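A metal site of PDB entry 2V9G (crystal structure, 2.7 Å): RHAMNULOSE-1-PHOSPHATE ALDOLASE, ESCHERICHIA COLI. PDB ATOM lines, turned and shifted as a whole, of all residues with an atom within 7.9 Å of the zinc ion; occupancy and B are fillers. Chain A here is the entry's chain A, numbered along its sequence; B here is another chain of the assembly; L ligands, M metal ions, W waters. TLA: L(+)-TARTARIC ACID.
Within 4 Å of the zinc ion: His 141, His 143 and His 212.
The nearest printed residue that does not touch the zinc ion is Gly 31 (4.2 Å).
The backbone carbonyl oxygen (O) of His 141 lies within hydrogen-bond range of the backbone NH (N) of Asn 32 (2.8 Å).
The backbone carbonyl oxygen (O) of Val 214 lies within hydrogen-bond range of a ring nitrogen (ND1) of His 141, at 2.9 Å.
OE2 of Glu 171 of chain B lies within hydrogen-bond range of ND1 of His 143, 3.0 Å away.
The side-chain carboxylate (OE1) of Glu 27 lies within hydrogen-bond range of a ring nitrogen (ND1) of His 143 (2.9 Å).
The backbone carbonyl oxygen (O) of Trp 25 lies within hydrogen-bond range of the backbone NH (N) of His 143 (2.9 Å).
The zinc ion is bound by water W1, NE2 of His 212, NE2 of His 141, NE2 of His 143 and O3 of the ligand.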
ATOM      1  N   TRP A  25      19.456  17.092 -10.007  1.00  0.00           N
ATOM      2  CA  TRP A  25      19.629  18.401 -10.642  1.00  0.00           C
ATOM      3  C   TRP A  25      21.026  18.621 -11.189  1.00  0.00           C
ATOM      4  O   TRP A  25      21.338  19.693 -11.701  1.00  0.00           O
ATOM      5  CB  TRP A  25      19.398  19.536  -9.636  1.00  0.00           C
ATOM      6  CG  TRP A  25      18.114  19.536  -8.894  1.00  0.00           C
ATOM      7  CD1 TRP A  25      16.929  19.000  -9.294  1.00  0.00           C
ATOM      8  CD2 TRP A  25      17.866  20.187  -7.648  1.00  0.00           C
ATOM      9  NE1 TRP A  25      15.951  19.266  -8.359  1.00  0.00           N
ATOM     10  CE2 TRP A  25      16.501  19.994  -7.342  1.00  0.00           C
ATOM     11  CE3 TRP A  25      18.669  20.909  -6.757  1.00  0.00           C
ATOM     12  CZ2 TRP A  25      15.924  20.499  -6.186  1.00  0.00           C
ATOM     13  CZ3 TRP A  25      18.094  21.419  -5.618  1.00  0.00           C
ATOM     14  CH2 TRP A  25      16.734  21.216  -5.331  1.00  0.00           C
ATOM     15  N   ASP A  26      21.907  17.628 -11.066  1.00  0.00           N
ATOM     16  CA  ASP A  26      23.267  17.856 -11.544  1.00  0.00           C
ATOM     17  C   ASP A  26      23.997  16.666 -12.134  1.00  0.00           C
ATOM     18  O   ASP A  26      24.832  16.033 -11.494  1.00  0.00           O
ATOM     19  CB  ASP A  26      24.092  18.477 -10.429  1.00  0.00           C
ATOM     20  CG  ASP A  26      23.568  19.848 -10.012  1.00  0.00           C
ATOM     21  OD1 ASP A  26      22.642  19.933  -9.185  1.00  0.00           O
ATOM     22  OD2 ASP A  26      24.075  20.854 -10.545  1.00  0.00           O
ATOM     23  N   GLU A  27      23.699  16.382 -13.397  1.00  0.00           N
ATOM     24  CA  GLU A  27      24.326  15.287 -14.108  1.00  0.00           C
ATOM     25  C   GLU A  27      25.718  15.736 -14.496  1.00  0.00           C
ATOM     26  O   GLU A  27      26.010  16.948 -14.466  1.00  0.00           O
ATOM     27  CB  GLU A  27      23.544  14.954 -15.379  1.00  0.00           C
ATOM     28  CG  GLU A  27      23.577  16.075 -16.413  1.00  0.00           C
ATOM     29  CD  GLU A  27      22.727  17.258 -16.018  1.00  0.00           C
ATOM     30  OE1 GLU A  27      22.863  18.318 -16.649  1.00  0.00           O
ATOM     31  OE2 GLU A  27      21.905  17.111 -15.088  1.00  0.00           O
ATOM     32  N   ASN A  29      28.994  17.249 -15.063  1.00  0.00           N
ATOM     33  CA  ASN A  29      29.615  18.378 -14.404  1.00  0.00           C
ATOM     34  C   ASN A  29      28.611  19.522 -14.227  1.00  0.00           C
ATOM     35  O   ASN A  29      28.965  20.614 -13.782  1.00  0.00           O
ATOM     36  CB  ASN A  29      30.777  18.865 -15.264  1.00  0.00           C
ATOM     37  CG  ASN A  29      30.301  19.551 -16.512  1.00  0.00           C
ATOM     38  OD1 ASN A  29      29.499  18.994 -17.282  1.00  0.00           O
ATOM     39  ND2 ASN A  29      30.768  20.786 -16.730  1.00  0.00           N
ATOM     40  N   GLY A  30      27.365  19.272 -14.611  1.00  0.00           N
ATOM     41  CA  GLY A  30      26.347  20.299 -14.480  1.00  0.00           C
ATOM     42  C   GLY A  30      26.253  20.870 -13.079  1.00  0.00           C
ATOM     43  O   GLY A  30      26.445  20.161 -12.085  1.00  0.00           O
ATOM     44  N   GLY A  31      25.964  22.175 -13.007  1.00  0.00           N
ATOM     45  CA  GLY A  31      25.828  22.861 -11.734  1.00  0.00           C
ATOM     46  C   GLY A  31      27.150  23.280 -11.119  1.00  0.00           C
ATOM     47  O   GLY A  31      28.222  22.771 -11.483  1.00  0.00           O
ATOM     48  N   ASN A  32      27.088  24.241 -10.198  1.00  0.00           N
ATOM     49  CA  ASN A  32      28.272  24.720  -9.490  1.00  0.00           C
ATOM     50  C   ASN A  32      27.784  25.492  -8.275  1.00  0.00           C
ATOM     51  O   ASN A  32      26.644  25.957  -8.251  1.00  0.00           O
ATOM     52  CB  ASN A  32      29.130  25.587 -10.407  1.00  0.00           C
ATOM     53  CG  ASN A  32      28.325  26.506 -11.276  1.00  0.00           C
ATOM     54  OD1 ASN A  32      27.588  27.349 -10.778  1.00  0.00           O
ATOM     55  ND2 ASN A  32      28.449  26.344 -12.580  1.00  0.00           N
ATOM     56  N   THR A 115      34.978  26.677 -10.985  1.00  0.00           N
ATOM     57  CA  THR A 115      33.937  26.516 -12.015  1.00  0.00           C
ATOM     58  C   THR A 115      34.020  27.606 -13.075  1.00  0.00           C
ATOM     59  O   THR A 115      34.430  28.729 -12.806  1.00  0.00           O
ATOM     60  CB  THR A 115      32.504  26.608 -11.449  1.00  0.00           C
ATOM     61  OG1 THR A 115      31.562  26.614 -12.537  1.00  0.00           O
ATOM     62  CG2 THR A 115      32.330  27.890 -10.647  1.00  0.00           C
ATOM     63  N   SER A 116      33.595  27.237 -14.276  1.00  0.00           N
ATOM     64  CA  SER A 116      33.603  28.154 -15.407  1.00  0.00           C
ATOM     65  C   SER A 116      32.572  29.286 -15.230  1.00  0.00           C
ATOM     66  O   SER A 116      32.651  30.318 -15.904  1.00  0.00           O
ATOM     67  CB  SER A 116      33.320  27.372 -16.686  1.00  0.00           C
ATOM     68  OG  SER A 116      32.283  26.425 -16.476  1.00  0.00           O
ATOM     69  N   GLU A 117      31.615  29.107 -14.317  1.00  0.00           N
ATOM     70  CA  GLU A 117      30.628  30.162 -14.087  1.00  0.00           C
ATOM     71  C   GLU A 117      31.083  31.061 -12.946  1.00  0.00           C
ATOM     72  O   GLU A 117      30.271  31.759 -12.341  1.00  0.00           O
ATOM     73  CB  GLU A 117      29.245  29.581 -13.757  1.00  0.00           C
ATOM     74  CG  GLU A 117      28.646  28.652 -14.833  1.00  0.00           C
ATOM     75  CD  GLU A 117      28.319  29.322 -16.167  1.00  0.00           C
ATOM     76  OE1 GLU A 117      27.895  28.595 -17.086  1.00  0.00           O
ATOM     77  OE2 GLU A 117      28.484  30.550 -16.309  1.00  0.00           O
ATOM     78  N   HIS A 141      24.084  27.287  -8.579  1.00  0.00           N
ATOM     79  CA  HIS A 141      23.578  27.013  -9.912  1.00  0.00           C
ATOM     80  C   HIS A 141      23.409  25.506 -10.084  1.00  0.00           C
ATOM     81  O   HIS A 141      24.313  24.720  -9.774  1.00  0.00           O
ATOM     82  CB  HIS A 141      24.526  27.559 -10.980  1.00  0.00           C
ATOM     83  CG  HIS A 141      24.252  27.024 -12.351  1.00  0.00           C
ATOM     84  ND1 HIS A 141      23.023  27.147 -12.963  1.00  0.00           N
ATOM     85  CD2 HIS A 141      25.034  26.346 -13.217  1.00  0.00           C
ATOM     86  CE1 HIS A 141      23.053  26.564 -14.147  1.00  0.00           C
ATOM     87  NE2 HIS A 141      24.270  26.071 -14.330  1.00  0.00           N
ATOM     88  N   CYS A 142      22.243  25.106 -10.558  1.00  0.00           N
ATOM     89  CA  CYS A 142      22.011  23.703 -10.821  1.00  0.00           C
ATOM     90  C   CYS A 142      20.931  23.592 -11.880  1.00  0.00           C
ATOM     91  O   CYS A 142      20.174  24.542 -12.123  1.00  0.00           O
ATOM     92  CB  CYS A 142      21.591  22.967  -9.548  1.00  0.00           C
ATOM     93  SG  CYS A 142      19.971  23.393  -8.976  1.00  0.00           S
ATOM     94  N   HIS A 143      20.891  22.435 -12.506  1.00  0.00           N
ATOM     95  CA  HIS A 143      19.958  22.159 -13.568  1.00  0.00           C
ATOM     96  C   HIS A 143      18.700  21.523 -13.021  1.00  0.00           C
ATOM     97  O   HIS A 143      18.479  20.326 -13.171  1.00  0.00           O
ATOM     98  CB  HIS A 143      20.638  21.270 -14.596  1.00  0.00           C
ATOM     99  CG  HIS A 143      21.914  21.856 -15.134  1.00  0.00           C
ATOM    100  ND1 HIS A 143      22.864  21.098 -15.801  1.00  0.00           N
ATOM    101  CD2 HIS A 143      22.368  23.128 -15.160  1.00  0.00           C
ATOM    102  CE1 HIS A 143      23.836  21.884 -16.211  1.00  0.00           C
ATOM    103  NE2 HIS A 143      23.565  23.122 -15.836  1.00  0.00           N
ATOM    104  N   PRO A 188      26.711  30.296 -22.401  1.00  0.00           N
ATOM    105  CA  PRO A 188      27.226  30.177 -21.032  1.00  0.00           C
ATOM    106  C   PRO A 188      28.700  30.419 -20.748  1.00  0.00           C
ATOM    107  O   PRO A 188      29.526  30.517 -21.653  1.00  0.00           O
ATOM    108  CB  PRO A 188      26.799  28.767 -20.640  1.00  0.00           C
ATOM    109  CG  PRO A 188      26.882  28.025 -21.932  1.00  0.00           C
ATOM    110  CD  PRO A 188      26.257  28.988 -22.907  1.00  0.00           C
ATOM    111  N   GLY A 189      29.007  30.515 -19.456  1.00  0.00           N
ATOM    112  CA  GLY A 189      30.376  30.715 -19.016  1.00  0.00           C
ATOM    113  C   GLY A 189      31.066  31.972 -19.518  1.00  0.00           C
ATOM    114  O   GLY A 189      32.277  32.099 -19.381  1.00  0.00           O
ATOM    115  N   TRP A 209      17.790  30.400 -16.354  1.00  0.00           N
ATOM    116  CA  TRP A 209      18.515  30.451 -17.609  1.00  0.00           C
ATOM    117  C   TRP A 209      17.788  29.477 -18.531  1.00  0.00           C
ATOM    118  O   TRP A 209      18.001  28.280 -18.444  1.00  0.00           O
ATOM    119  CB  TRP A 209      19.966  29.996 -17.439  1.00  0.00           C
ATOM    120  CG  TRP A 209      20.886  30.995 -16.799  1.00  0.00           C
ATOM    121  CD1 TRP A 209      20.578  32.259 -16.369  1.00  0.00           C
ATOM    122  CD2 TRP A 209      22.283  30.811 -16.532  1.00  0.00           C
ATOM    123  NE1 TRP A 209      21.698  32.870 -15.852  1.00  0.00           N
ATOM    124  CE2 TRP A 209      22.751  32.009 -15.942  1.00  0.00           C
ATOM    125  CE3 TRP A 209      23.178  29.758 -16.737  1.00  0.00           C
ATOM    126  CZ2 TRP A 209      24.079  32.178 -15.561  1.00  0.00           C
ATOM    127  CZ3 TRP A 209      24.496  29.918 -16.360  1.00  0.00           C
ATOM    128  CH2 TRP A 209      24.937  31.126 -15.770  1.00  0.00           C
ATOM    129  N   HIS A 212      18.446  25.754 -19.664  1.00  0.00           N
ATOM    130  CA  HIS A 212      19.706  25.506 -18.987  1.00  0.00           C
ATOM    131  C   HIS A 212      19.514  25.202 -17.505  1.00  0.00           C
ATOM    132  O   HIS A 212      19.697  24.067 -17.075  1.00  0.00           O
ATOM    133  CB  HIS A 212      20.655  26.691 -19.183  1.00  0.00           C
ATOM    134  CG  HIS A 212      22.023  26.473 -18.635  1.00  0.00           C
ATOM    135  ND1 HIS A 212      23.125  27.184 -19.070  1.00  0.00           N
ATOM    136  CD2 HIS A 212      22.470  25.636 -17.670  1.00  0.00           C
ATOM    137  CE1 HIS A 212      24.192  26.794 -18.394  1.00  0.00           C
ATOM    138  NE2 HIS A 212      23.824  25.853 -17.538  1.00  0.00           N
ATOM    139  N   GLY A 213      19.176  26.206 -16.727  1.00  0.00           N
ATOM    140  CA  GLY A 213      19.000  25.940 -15.306  1.00  0.00           C
ATOM    141  C   GLY A 213      18.573  27.126 -14.485  1.00  0.00           C
ATOM    142  O   GLY A 213      17.949  28.046 -15.005  1.00  0.00           O
ATOM    143  N   VAL A 214      18.902  27.104 -13.205  1.00  0.00           N
ATOM    144  CA  VAL A 214      18.522  28.181 -12.319  1.00  0.00           C
ATOM    145  C   VAL A 214      19.715  28.671 -11.518  1.00  0.00           C
ATOM    146  O   VAL A 214      20.705  27.956 -11.373  1.00  0.00           O
ATOM    147  CB  VAL A 214      17.428  27.702 -11.342  1.00  0.00           C
ATOM    148  CG1 VAL A 214      17.998  26.597 -10.430  1.00  0.00           C
ATOM    149  CG2 VAL A 214      16.912  28.852 -10.528  1.00  0.00           C
ATOM    150  N   PHE A 215      19.611  29.899 -11.030  1.00  0.00           N
ATOM    151  CA  PHE A 215      20.665  30.519 -10.222  1.00  0.00           C
ATOM    152  C   PHE A 215      20.014  31.038  -8.941  1.00  0.00           C
ATOM    153  O   PHE A 215      19.015  31.757  -9.003  1.00  0.00           O
ATOM    154  CB  PHE A 215      21.296  31.686 -10.972  1.00  0.00           C
ATOM    155  CG  PHE A 215      22.753  31.503 -11.258  1.00  0.00           C
ATOM    156  CD1 PHE A 215      23.171  30.718 -12.323  1.00  0.00           C
ATOM    157  CD2 PHE A 215      23.705  32.115 -10.458  1.00  0.00           C
ATOM    158  CE1 PHE A 215      24.530  30.536 -12.591  1.00  0.00           C
ATOM    159  CE2 PHE A 215      25.062  31.947 -10.722  1.00  0.00           C
ATOM    160  CZ  PHE A 215      25.469  31.154 -11.791  1.00  0.00           C
ATOM    161  N   THR B 170      21.349  22.887 -22.715  1.00  0.00           N
ATOM    162  CA  THR B 170      22.463  23.679 -23.249  1.00  0.00           C
ATOM    163  C   THR B 170      23.820  22.989 -23.322  1.00  0.00           C
ATOM    164  O   THR B 170      24.539  23.121 -24.304  1.00  0.00           O
ATOM    165  CB  THR B 170      22.647  24.964 -22.422  1.00  0.00           C
ATOM    166  OG1 THR B 170      21.464  25.774 -22.503  1.00  0.00           O
ATOM    167  CG2 THR B 170      23.836  25.752 -22.948  1.00  0.00           C
ATOM    168  N   GLU B 171      24.150  22.247 -22.272  1.00  0.00           N
ATOM    169  CA  GLU B 171      25.435  21.561 -22.180  1.00  0.00           C
ATOM    170  C   GLU B 171      25.635  20.480 -23.225  1.00  0.00           C
ATOM    171  O   GLU B 171      26.756  20.262 -23.679  1.00  0.00           O
ATOM    172  CB  GLU B 171      25.574  20.917 -20.803  1.00  0.00           C
ATOM    173  CG  GLU B 171      24.490  19.876 -20.560  1.00  0.00           C
ATOM    174  CD  GLU B 171      24.383  19.400 -19.131  1.00  0.00           C
ATOM    175  OE1 GLU B 171      25.230  18.577 -18.688  1.00  0.00           O
ATOM    176  OE2 GLU B 171      23.449  19.857 -18.446  1.00  0.00           O
HETATM  177  O1  TLA L   1      26.018  24.035 -18.699  1.00  0.00           O
HETATM  178  O11 TLA L   1      28.117  24.579 -19.304  1.00  0.00           O
HETATM  179  C1  TLA L   1      27.257  24.081 -18.506  1.00  0.00           C
HETATM  180  C2  TLA L   1      27.795  23.478 -17.220  1.00  0.00           C
HETATM  181  O2  TLA L   1      26.762  22.785 -16.535  1.00  0.00           O
HETATM  182  C3  TLA L   1      28.368  24.542 -16.290  1.00  0.00           C
HETATM  183  O3  TLA L   1      27.414  25.512 -16.010  1.00  0.00           O
HETATM  184  C4  TLA L   1      28.905  23.834 -15.064  1.00  0.00           C
HETATM  185  O4  TLA L   1      28.145  23.812 -14.051  1.00  0.00           O
HETATM  186  O41 TLA L   1      30.034  23.301 -15.123  1.00  0.00           O
HETATM  187 ZN    ZN M   1      24.981  25.002 -16.015  1.00  0.00          ZN
HETATM  188  O   HOH W   1      25.417  23.861 -14.369  1.00  0.00           O
